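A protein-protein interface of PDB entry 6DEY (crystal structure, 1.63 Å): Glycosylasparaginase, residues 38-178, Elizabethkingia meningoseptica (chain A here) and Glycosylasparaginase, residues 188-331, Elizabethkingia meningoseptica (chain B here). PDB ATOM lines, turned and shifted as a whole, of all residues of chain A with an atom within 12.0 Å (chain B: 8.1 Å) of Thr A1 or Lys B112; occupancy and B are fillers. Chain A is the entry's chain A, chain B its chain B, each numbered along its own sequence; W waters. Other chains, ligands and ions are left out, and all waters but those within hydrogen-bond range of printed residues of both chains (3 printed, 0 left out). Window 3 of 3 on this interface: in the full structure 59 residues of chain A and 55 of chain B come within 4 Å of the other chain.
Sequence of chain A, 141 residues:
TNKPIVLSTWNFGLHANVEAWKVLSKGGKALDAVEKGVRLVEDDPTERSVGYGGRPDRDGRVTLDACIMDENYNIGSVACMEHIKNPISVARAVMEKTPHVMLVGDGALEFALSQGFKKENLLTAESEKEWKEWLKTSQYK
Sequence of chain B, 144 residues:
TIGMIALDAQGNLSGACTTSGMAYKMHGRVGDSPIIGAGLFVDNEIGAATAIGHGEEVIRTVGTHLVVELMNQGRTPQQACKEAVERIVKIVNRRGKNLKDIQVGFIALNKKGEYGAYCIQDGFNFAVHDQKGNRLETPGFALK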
ATOM      1  N   THR A   1      26.480 -15.845 -16.696  1.00  0.00           N
ATOM      2  CA  THR A   1      25.915 -14.978 -15.601  1.00  0.00           C
ATOM      3  C   THR A   1      26.750 -15.126 -14.343  1.00  0.00           C
ATOM      4  O   THR A   1      26.968 -16.254 -13.910  1.00  0.00           O
ATOM      5  CB  THR A   1      24.433 -15.333 -15.340  1.00  0.00           C
ATOM      6  OG1 THR A   1      23.653 -14.788 -16.391  1.00  0.00           O
ATOM      7  CG2 THR A   1      23.881 -14.757 -14.105  1.00  0.00           C
ATOM      8  N   ASN A   2      27.237 -14.004 -13.779  1.00  0.00           N
ATOM      9  CA  ASN A   2      28.055 -13.972 -12.603  1.00  0.00           C
ATOM     10  C   ASN A   2      27.102 -13.760 -11.453  1.00  0.00           C
ATOM     11  O   ASN A   2      26.765 -12.608 -11.174  1.00  0.00           O
ATOM     12  CB  ASN A   2      29.005 -12.766 -12.645  1.00  0.00           C
ATOM     13  CG  ASN A   2      29.993 -12.704 -11.481  1.00  0.00           C
ATOM     14  OD1 ASN A   2      30.243 -13.699 -10.790  1.00  0.00           O
ATOM     15  ND2 ASN A   2      30.488 -11.502 -11.180  1.00  0.00           N
ATOM     16  N   LYS A   3      26.746 -14.821 -10.754  1.00  0.00           N
ATOM     17  CA  LYS A   3      25.888 -14.719  -9.594  1.00  0.00           C
ATOM     18  C   LYS A   3      26.230 -15.805  -8.614  1.00  0.00           C
ATOM     19  O   LYS A   3      26.671 -16.917  -9.030  1.00  0.00           O
ATOM     20  CB  LYS A   3      24.390 -14.844 -10.014  1.00  0.00           C
ATOM     21  CG  LYS A   3      23.972 -16.213 -10.483  1.00  0.00           C
ATOM     22  CD  LYS A   3      22.539 -16.201 -11.008  1.00  0.00           C
ATOM     23  CE  LYS A   3      22.373 -17.241 -12.114  1.00  0.00           C
ATOM     24  NZ  LYS A   3      21.216 -18.080 -11.823  1.00  0.00           N
ATOM     25  N   PRO A   4      26.032 -15.643  -7.330  1.00  0.00           N
ATOM     26  CA  PRO A   4      25.605 -14.386  -6.750  1.00  0.00           C
ATOM     27  C   PRO A   4      26.677 -13.312  -6.727  1.00  0.00           C
ATOM     28  O   PRO A   4      27.867 -13.586  -6.886  1.00  0.00           O
ATOM     29  CB  PRO A   4      25.275 -14.758  -5.314  1.00  0.00           C
ATOM     30  CG  PRO A   4      25.950 -16.040  -5.009  1.00  0.00           C
ATOM     31  CD  PRO A   4      26.306 -16.682  -6.316  1.00  0.00           C
ATOM     32  N   ILE A   5      26.228 -12.049  -6.568  1.00  0.00           N
ATOM     33  CA  ILE A   5      27.159 -10.931  -6.510  1.00  0.00           C
ATOM     34  C   ILE A   5      26.441  -9.856  -5.677  1.00  0.00           C
ATOM     35  O   ILE A   5      25.208  -9.678  -5.861  1.00  0.00           O
ATOM     36  CB  ILE A   5      27.571 -10.394  -7.924  1.00  0.00           C
ATOM     37  CG1 ILE A   5      28.455  -9.120  -7.787  1.00  0.00           C
ATOM     38  CG2 ILE A   5      26.384 -10.163  -8.788  1.00  0.00           C
ATOM     39  CD1 ILE A   5      29.235  -8.825  -9.056  1.00  0.00           C
ATOM     40  N   VAL A   6      27.204  -9.155  -4.872  1.00  0.00           N
ATOM     41  CA  VAL A   6      26.688  -7.996  -4.089  1.00  0.00           C
ATOM     42  C   VAL A   6      27.635  -6.860  -4.205  1.00  0.00           C
ATOM     43  O   VAL A   6      28.874  -7.061  -4.171  1.00  0.00           O
ATOM     44  CB  VAL A   6      26.413  -8.359  -2.617  1.00  0.00           C
ATOM     45  CG1 VAL A   6      27.634  -8.944  -1.899  1.00  0.00           C
ATOM     46  CG2 VAL A   6      25.956  -7.208  -1.777  1.00  0.00           C
ATOM     47  N   LEU A   7      27.101  -5.632  -4.317  1.00  0.00           N
ATOM     48  CA  LEU A   7      27.867  -4.376  -4.325  1.00  0.00           C
ATOM     49  C   LEU A   7      27.350  -3.488  -3.225  1.00  0.00           C
ATOM     50  O   LEU A   7      26.133  -3.442  -2.972  1.00  0.00           O
ATOM     51  CB  LEU A   7      27.688  -3.584  -5.624  1.00  0.00           C
ATOM     52  CG  LEU A   7      28.699  -3.869  -6.765  1.00  0.00           C
ATOM     53  CD1 LEU A   7      28.489  -5.222  -7.301  1.00  0.00           C
ATOM     54  CD2 LEU A   7      28.603  -2.779  -7.838  1.00  0.00           C
ATOM     55  N   TRP A  21      27.038 -11.959   2.118  1.00  0.00           N
ATOM     56  CA  TRP A  21      27.562 -13.131   1.437  1.00  0.00           C
ATOM     57  C   TRP A  21      27.209 -14.394   2.304  1.00  0.00           C
ATOM     58  O   TRP A  21      27.037 -15.487   1.716  1.00  0.00           O
ATOM     59  CB  TRP A  21      29.068 -13.055   1.243  1.00  0.00           C
ATOM     60  CG  TRP A  21      29.537 -14.049   0.259  1.00  0.00           C
ATOM     61  CD1 TRP A  21      30.340 -15.169   0.528  1.00  0.00           C
ATOM     62  CD2 TRP A  21      29.343 -14.022  -1.176  1.00  0.00           C
ATOM     63  NE1 TRP A  21      30.614 -15.822  -0.658  1.00  0.00           N
ATOM     64  CE2 TRP A  21      29.993 -15.178  -1.717  1.00  0.00           C
ATOM     65  CE3 TRP A  21      28.665 -13.166  -2.066  1.00  0.00           C
ATOM     66  CZ2 TRP A  21      30.009 -15.447  -3.030  1.00  0.00           C
ATOM     67  CZ3 TRP A  21      28.661 -13.479  -3.450  1.00  0.00           C
ATOM     68  CH2 TRP A  21      29.329 -14.631  -3.900  1.00  0.00           C
ATOM     69  N   LEU A  24      23.986 -15.056   0.695  1.00  0.00           N
ATOM     70  CA  LEU A  24      23.978 -15.304  -0.712  1.00  0.00           C
ATOM     71  C   LEU A  24      24.734 -16.623  -1.104  1.00  0.00           C
ATOM     72  O   LEU A  24      24.332 -17.345  -2.017  1.00  0.00           O
ATOM     73  CB  LEU A  24      24.636 -14.140  -1.465  1.00  0.00           C
ATOM     74  CG  LEU A  24      23.931 -12.789  -1.499  1.00  0.00           C
ATOM     75  CD1 LEU A  24      24.820 -11.659  -2.010  1.00  0.00           C
ATOM     76  CD2 LEU A  24      22.704 -12.848  -2.358  1.00  0.00           C
ATOM     77  N   LEU B   7      22.467  -9.578  -6.502  1.00  0.00           N
ATOM     78  CA  LEU B   7      21.914 -10.566  -7.428  1.00  0.00           C
ATOM     79  C   LEU B   7      22.132 -11.942  -6.810  1.00  0.00           C
ATOM     80  O   LEU B   7      23.277 -12.334  -6.497  1.00  0.00           O
ATOM     81  CB  LEU B   7      22.631 -10.514  -8.763  1.00  0.00           C
ATOM     82  CG  LEU B   7      22.133 -11.458  -9.838  1.00  0.00           C
ATOM     83  CD1 LEU B   7      20.723 -11.113 -10.367  1.00  0.00           C
ATOM     84  CD2 LEU B   7      23.070 -11.408 -11.013  1.00  0.00           C
ATOM     85  N   ASP B   8      21.076 -12.660  -6.496  1.00  0.00           N
ATOM     86  CA  ASP B   8      21.159 -13.962  -5.749  1.00  0.00           C
ATOM     87  C   ASP B   8      21.292 -15.135  -6.731  1.00  0.00           C
ATOM     88  O   ASP B   8      21.328 -14.950  -7.970  1.00  0.00           O
ATOM     89  CB  ASP B   8      20.013 -14.057  -4.727  1.00  0.00           C
ATOM     90  CG  ASP B   8      18.683 -14.172  -5.341  1.00  0.00           C
ATOM     91  OD1 ASP B   8      18.560 -14.608  -6.467  1.00  0.00           O
ATOM     92  OD2 ASP B   8      17.683 -13.862  -4.645  1.00  0.00           O
ATOM     93  N   ALA B   9      21.432 -16.306  -6.135  1.00  0.00           N
ATOM     94  CA  ALA B   9      21.656 -17.539  -6.926  1.00  0.00           C
ATOM     95  C   ALA B   9      20.474 -17.868  -7.797  1.00  0.00           C
ATOM     96  O   ALA B   9      20.633 -18.532  -8.825  1.00  0.00           O
ATOM     97  CB  ALA B   9      21.932 -18.720  -6.054  1.00  0.00           C
ATOM     98  N   GLN B  10      19.295 -17.388  -7.485  1.00  0.00           N
ATOM     99  CA  GLN B  10      18.122 -17.508  -8.378  1.00  0.00           C
ATOM    100  C   GLN B  10      18.097 -16.526  -9.538  1.00  0.00           C
ATOM    101  O   GLN B  10      17.259 -16.613 -10.450  1.00  0.00           O
ATOM    102  CB  GLN B  10      16.831 -17.319  -7.639  1.00  0.00           C
ATOM    103  CG  GLN B  10      16.503 -18.359  -6.639  1.00  0.00           C
ATOM    104  CD  GLN B  10      15.489 -17.800  -5.659  1.00  0.00           C
ATOM    105  OE1 GLN B  10      15.892 -17.331  -4.557  1.00  0.00           O
ATOM    106  NE2 GLN B  10      14.211 -17.805  -6.062  1.00  0.00           N
ATOM    107  N   GLY B  11      18.976 -15.533  -9.539  1.00  0.00           N
ATOM    108  CA  GLY B  11      19.027 -14.540 -10.548  1.00  0.00           C
ATOM    109  C   GLY B  11      18.049 -13.394 -10.242  1.00  0.00           C
ATOM    110  O   GLY B  11      17.657 -12.666 -11.133  1.00  0.00           O
ATOM    111  N   LEU B  13      17.261  -9.787  -8.189  1.00  0.00           N
ATOM    112  CA  LEU B  13      17.839  -8.582  -7.619  1.00  0.00           C
ATOM    113  C   LEU B  13      17.048  -8.108  -6.423  1.00  0.00           C
ATOM    114  O   LEU B  13      15.878  -8.252  -6.353  1.00  0.00           O
ATOM    115  CB  LEU B  13      17.888  -7.496  -8.653  1.00  0.00           C
ATOM    116  CG  LEU B  13      18.820  -7.740  -9.824  1.00  0.00           C
ATOM    117  CD1 LEU B  13      18.409  -6.784 -10.971  1.00  0.00           C
ATOM    118  CD2 LEU B  13      20.221  -7.365  -9.452  1.00  0.00           C
ATOM    119  N   GLU B  45      13.857  -7.160 -14.354  1.00  0.00           N
ATOM    120  CA  GLU B  45      14.076  -7.438 -15.769  1.00  0.00           C
ATOM    121  C   GLU B  45      15.260  -6.674 -16.344  1.00  0.00           C
ATOM    122  O   GLU B  45      15.663  -6.934 -17.489  1.00  0.00           O
ATOM    123  CB  GLU B  45      12.849  -7.146 -16.651  1.00  0.00           C
ATOM    124  CG  GLU B  45      11.590  -7.854 -16.269  1.00  0.00           C
ATOM    125  CD  GLU B  45      11.768  -9.339 -16.382  1.00  0.00           C
ATOM    126  OE1 GLU B  45      12.235  -9.769 -17.440  1.00  0.00           O
ATOM    127  OE2 GLU B  45      11.471 -10.105 -15.431  1.00  0.00           O
ATOM    128  N   ILE B  46      15.879  -5.769 -15.572  1.00  0.00           N
ATOM    129  CA  ILE B  46      16.881  -4.871 -16.076  1.00  0.00           C
ATOM    130  C   ILE B  46      18.125  -4.809 -15.236  1.00  0.00           C
ATOM    131  O   ILE B  46      19.199  -5.106 -15.725  1.00  0.00           O
ATOM    132  CB  ILE B  46      16.320  -3.419 -16.191  1.00  0.00           C
ATOM    133  CG1 ILE B  46      14.958  -3.387 -16.998  1.00  0.00           C
ATOM    134  CG2 ILE B  46      17.387  -2.479 -16.692  1.00  0.00           C
ATOM    135  CD1 ILE B  46      14.179  -2.100 -16.819  1.00  0.00           C
ATOM    136  N   GLY B  47      17.958  -4.403 -13.983  1.00  0.00           N
ATOM    137  CA  GLY B  47      19.106  -4.105 -13.162  1.00  0.00           C
ATOM    138  C   GLY B  47      18.737  -3.330 -11.935  1.00  0.00           C
ATOM    139  O   GLY B  47      17.608  -3.067 -11.700  1.00  0.00           O
ATOM    140  N   PRO B  77      26.038  -1.669 -17.175  1.00  0.00           N
ATOM    141  CA  PRO B  77      26.073  -0.939 -15.882  1.00  0.00           C
ATOM    142  C   PRO B  77      27.061   0.189 -15.797  1.00  0.00           C
ATOM    143  O   PRO B  77      26.765   1.264 -15.369  1.00  0.00           O
ATOM    144  CB  PRO B  77      26.291  -2.037 -14.871  1.00  0.00           C
ATOM    145  CG  PRO B  77      25.674  -3.256 -15.481  1.00  0.00           C
ATOM    146  CD  PRO B  77      26.069  -3.127 -16.949  1.00  0.00           C
ATOM    147  N   LEU B 109      24.166  -2.829 -11.100  1.00  0.00           N
ATOM    148  CA  LEU B 109      24.250  -4.245 -11.395  1.00  0.00           C
ATOM    149  C   LEU B 109      23.192  -4.549 -12.465  1.00  0.00           C
ATOM    150  O   LEU B 109      22.100  -3.913 -12.477  1.00  0.00           O
ATOM    151  CB  LEU B 109      23.939  -4.999 -10.100  1.00  0.00           C
ATOM    152  CG  LEU B 109      24.341  -6.300  -9.647  1.00  0.00           C
ATOM    153  CD1 LEU B 109      25.781  -6.640 -10.076  1.00  0.00           C
ATOM    154  CD2 LEU B 109      24.047  -6.432  -8.162  1.00  0.00           C
ATOM    155  N   ASN B 110      23.454  -5.496 -13.377  1.00  0.00           N
ATOM    156  CA  ASN B 110      22.402  -6.007 -14.287  1.00  0.00           C
ATOM    157  C   ASN B 110      22.103  -7.435 -13.995  1.00  0.00           C
ATOM    158  O   ASN B 110      22.696  -8.026 -13.091  1.00  0.00           O
ATOM    159  CB  ASN B 110      22.669  -5.718 -15.757  1.00  0.00           C
ATOM    160  CG  ASN B 110      23.825  -6.508 -16.327  1.00  0.00           C
ATOM    161  OD1 ASN B 110      24.325  -7.425 -15.706  1.00  0.00           O
ATOM    162  ND2 ASN B 110      24.283  -6.076 -17.489  1.00  0.00           N
ATOM    163  N   LYS B 111      21.201  -8.025 -14.811  1.00  0.00           N
ATOM    164  CA  LYS B 111      20.803  -9.434 -14.621  1.00  0.00           C
ATOM    165  C   LYS B 111      21.853 -10.460 -14.945  1.00  0.00           C
ATOM    166  O   LYS B 111      21.707 -11.589 -14.484  1.00  0.00           O
ATOM    167  CB  LYS B 111      19.534  -9.723 -15.420  1.00  0.00           C
ATOM    168  CG  LYS B 111      18.357  -9.010 -14.911  1.00  0.00           C
ATOM    169  CD  LYS B 111      18.227  -8.936 -13.406  1.00  0.00           C
ATOM    170  CE  LYS B 111      17.980 -10.295 -12.768  1.00  0.00           C
ATOM    171  NZ  LYS B 111      16.715 -10.927 -13.090  1.00  0.00           N
ATOM    172  N   LYS B 112      22.848 -10.085 -15.732  1.00  0.00           N
ATOM    173  CA  LYS B 112      24.061 -10.881 -15.984  1.00  0.00           C
ATOM    174  C   LYS B 112      25.019 -10.905 -14.815  1.00  0.00           C
ATOM    175  O   LYS B 112      26.008 -11.618 -14.880  1.00  0.00           O
ATOM    176  CB  LYS B 112      24.756 -10.416 -17.269  1.00  0.00           C
ATOM    177  CG  LYS B 112      24.035 -10.778 -18.525  1.00  0.00           C
ATOM    178  CD  LYS B 112      24.957 -10.715 -19.770  1.00  0.00           C
ATOM    179  CE  LYS B 112      24.474 -11.601 -20.905  1.00  0.00           C
ATOM    180  NZ  LYS B 112      24.645 -10.894 -22.228  1.00  0.00           N
ATOM    181  N   GLY B 113      24.829 -10.042 -13.796  1.00  0.00           N
ATOM    182  CA  GLY B 113      25.832  -9.817 -12.801  1.00  0.00           C
ATOM    183  C   GLY B 113      27.040  -9.038 -13.274  1.00  0.00           C
ATOM    184  O   GLY B 113      28.055  -9.058 -12.584  1.00  0.00           O
ATOM    185  N   GLU B 114      26.919  -8.301 -14.364  1.00  0.00           N
ATOM    186  CA  GLU B 114      27.877  -7.302 -14.732  1.00  0.00           C
ATOM    187  C   GLU B 114      27.605  -6.091 -13.805  1.00  0.00           C
ATOM    188  O   GLU B 114      26.467  -5.875 -13.343  1.00  0.00           O
ATOM    189  CB  GLU B 114      27.696  -6.851 -16.135  1.00  0.00           C
ATOM    190  CG  GLU B 114      27.984  -8.011 -17.078  1.00  0.00           C
ATOM    191  CD  GLU B 114      27.637  -7.741 -18.523  1.00  0.00           C
ATOM    192  OE1 GLU B 114      26.790  -6.924 -18.910  1.00  0.00           O
ATOM    193  OE2 GLU B 114      28.245  -8.484 -19.345  1.00  0.00           O
ATOM    194  N   TYR B 115      28.625  -5.298 -13.532  1.00  0.00           N
ATOM    195  CA  TYR B 115      28.532  -4.206 -12.591  1.00  0.00           C
ATOM    196  C   TYR B 115      29.348  -3.022 -13.051  1.00  0.00           C
ATOM    197  O   TYR B 115      30.187  -3.102 -13.956  1.00  0.00           O
ATOM    198  CB  TYR B 115      28.948  -4.598 -11.158  1.00  0.00           C
ATOM    199  CG  TYR B 115      30.411  -4.936 -10.974  1.00  0.00           C
ATOM    200  CD1 TYR B 115      31.331  -3.951 -10.611  1.00  0.00           C
ATOM    201  CD2 TYR B 115      30.833  -6.242 -11.119  1.00  0.00           C
ATOM    202  CE1 TYR B 115      32.670  -4.288 -10.430  1.00  0.00           C
ATOM    203  CE2 TYR B 115      32.158  -6.584 -10.925  1.00  0.00           C
ATOM    204  CZ  TYR B 115      33.048  -5.598 -10.609  1.00  0.00           C
ATOM    205  OH  TYR B 115      34.380  -5.948 -10.374  1.00  0.00           O
ATOM    206  N   GLN B 131      32.110 -14.645  -6.665  1.00  0.00           N
ATOM    207  CA  GLN B 131      32.857 -15.901  -6.440  1.00  0.00           C
ATOM    208  C   GLN B 131      34.364 -15.671  -6.474  1.00  0.00           C
ATOM    209  O   GLN B 131      35.104 -16.525  -5.932  1.00  0.00           O
ATOM    210  CB  GLN B 131      32.415 -16.942  -7.448  1.00  0.00           C
ATOM    211  CG  GLN B 131      31.019 -17.488  -7.108  1.00  0.00           C
ATOM    212  CD  GLN B 131      30.240 -18.082  -8.324  1.00  0.00           C
ATOM    213  OE1 GLN B 131      30.635 -17.938  -9.501  1.00  0.00           O
ATOM    214  NE2 GLN B 131      29.152 -18.728  -8.040  1.00  0.00           N
HETATM  215  O   HOH W   1      29.526 -15.005  -8.346  1.00  0.00           O
HETATM  216  O   HOH W   2      21.844 -16.591  -3.228  1.00  0.00           O
HETATM  217  O   HOH W   3      30.743  -9.261 -13.218  1.00  0.00           O
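The backbone NH of Gly B113 sits at hydrogen-bond distance from the side-chain amide oxygen of Asn B110.
OD1 of Asn B110 sits at hydrogen-bond distance from N of Lys B112 (3.0 Å).
The side-chain amino group of Lys B111 sits at hydrogen-bond distance from the backbone carbonyl oxygen of Gly B11 (2.8 Å).
The backbone NH of Gly B11 sits at hydrogen-bond distance from the side-chain carboxylate of Asp B8, 3.2 Å away.
The side-chain carboxylate of Asp B8 is in hydrogen-bond range of the backbone NH of Gln B10 (3.1 Å).
Thr A1 touches Lys B112.
CD2 of Leu B7 touches O of Asn A2, 3.9 Å away.
Gly B113 touches Asn A2.
Gly B11 touches Lys A3 (N to CD, 3.9 Å).
Pro A4 touches Leu B7.
Leu B109 touches Ile A5.
CD1 of Ile A5 touches O of Gly B113, 3.7 Å away.
CD1 of Ile A5 touches CD2 of Tyr B115, 3.7 Å away.
Leu A7 touches Tyr B115 (CD2 to CB, 3.8 Å).
N of Gln B131 touches CH2 of Trp A21 (3.9 Å).
Water W1 lies within hydrogen-bond range of the backbone carbonyl oxygen of Pro A4 (2.6 Å), the side-chain amide oxygen of Asn A2 (2.9 Å) and the backbone NH of Gln B131 (3.1 Å).
Water W3 lies within hydrogen-bond range of the backbone carbonyl oxygen of Gly B113 and the side-chain amide nitrogen of Asn A2.
Water W2 bridges O of Leu A24 (2.9 Å) and N of Ala B9 (2.9 Å).
Of the 18 printed residues of chain B, 10 touch a printed residue of chain A.
Hydrophobic or aromatic side chains of chain B within 4 Å of the printed part of chain A: Leu B7, Leu B109 and Tyr B115.
Along chain B the printed residues that touch a printed residue of chain A span positions 7 to 131.
Among the printed residues, no Asp or Glu carboxylate lies within 4 Å of a Lys or Arg side-chain nitrogen of the other chain.
The backbone carbonyl oxygen of Lys A3 is in hydrogen-bond range of the side-chain amide nitrogen of Gln B131, at 3.2 Å.
The backbone carbonyl oxygen of Lys B112 lies within hydrogen-bond range of the backbone NH of Asn A2 (2.9 Å).
N of Leu B7 is in hydrogen-bond range of O of Ile A5 (2.8 Å).
O of Ala B9 lies within hydrogen-bond range of NZ of Lys A3 (3.1 Å).
Thr A1 touches just these residues of chain B: Lys B111 and Lys B112.
Of chain A, only Lys A3 (3.9 Å) comes within 4 Å of Gly B11.
Of chain A, only Thr A1 comes within 4 Å of Lys B111.
Of chain A, only Asn A2 (3.4 Å) and Ile A5 (3.7 Å) come within 4 Å of Gly B113.
No residue of chain A comes within 4 Å of Glu B114.
Of the printed residues of chain B, Pro A4 touches Leu B7 (3.1 Å) and Gln B131 (3.9 Å).
Of the printed residues of chain B, Lys A3 touches Leu B7, Asp B8, Ala B9, Gly B11 and Gln B131.
The nearest residue of chain B that does not touch Thr A1 is Leu B7 (4.6 Å).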
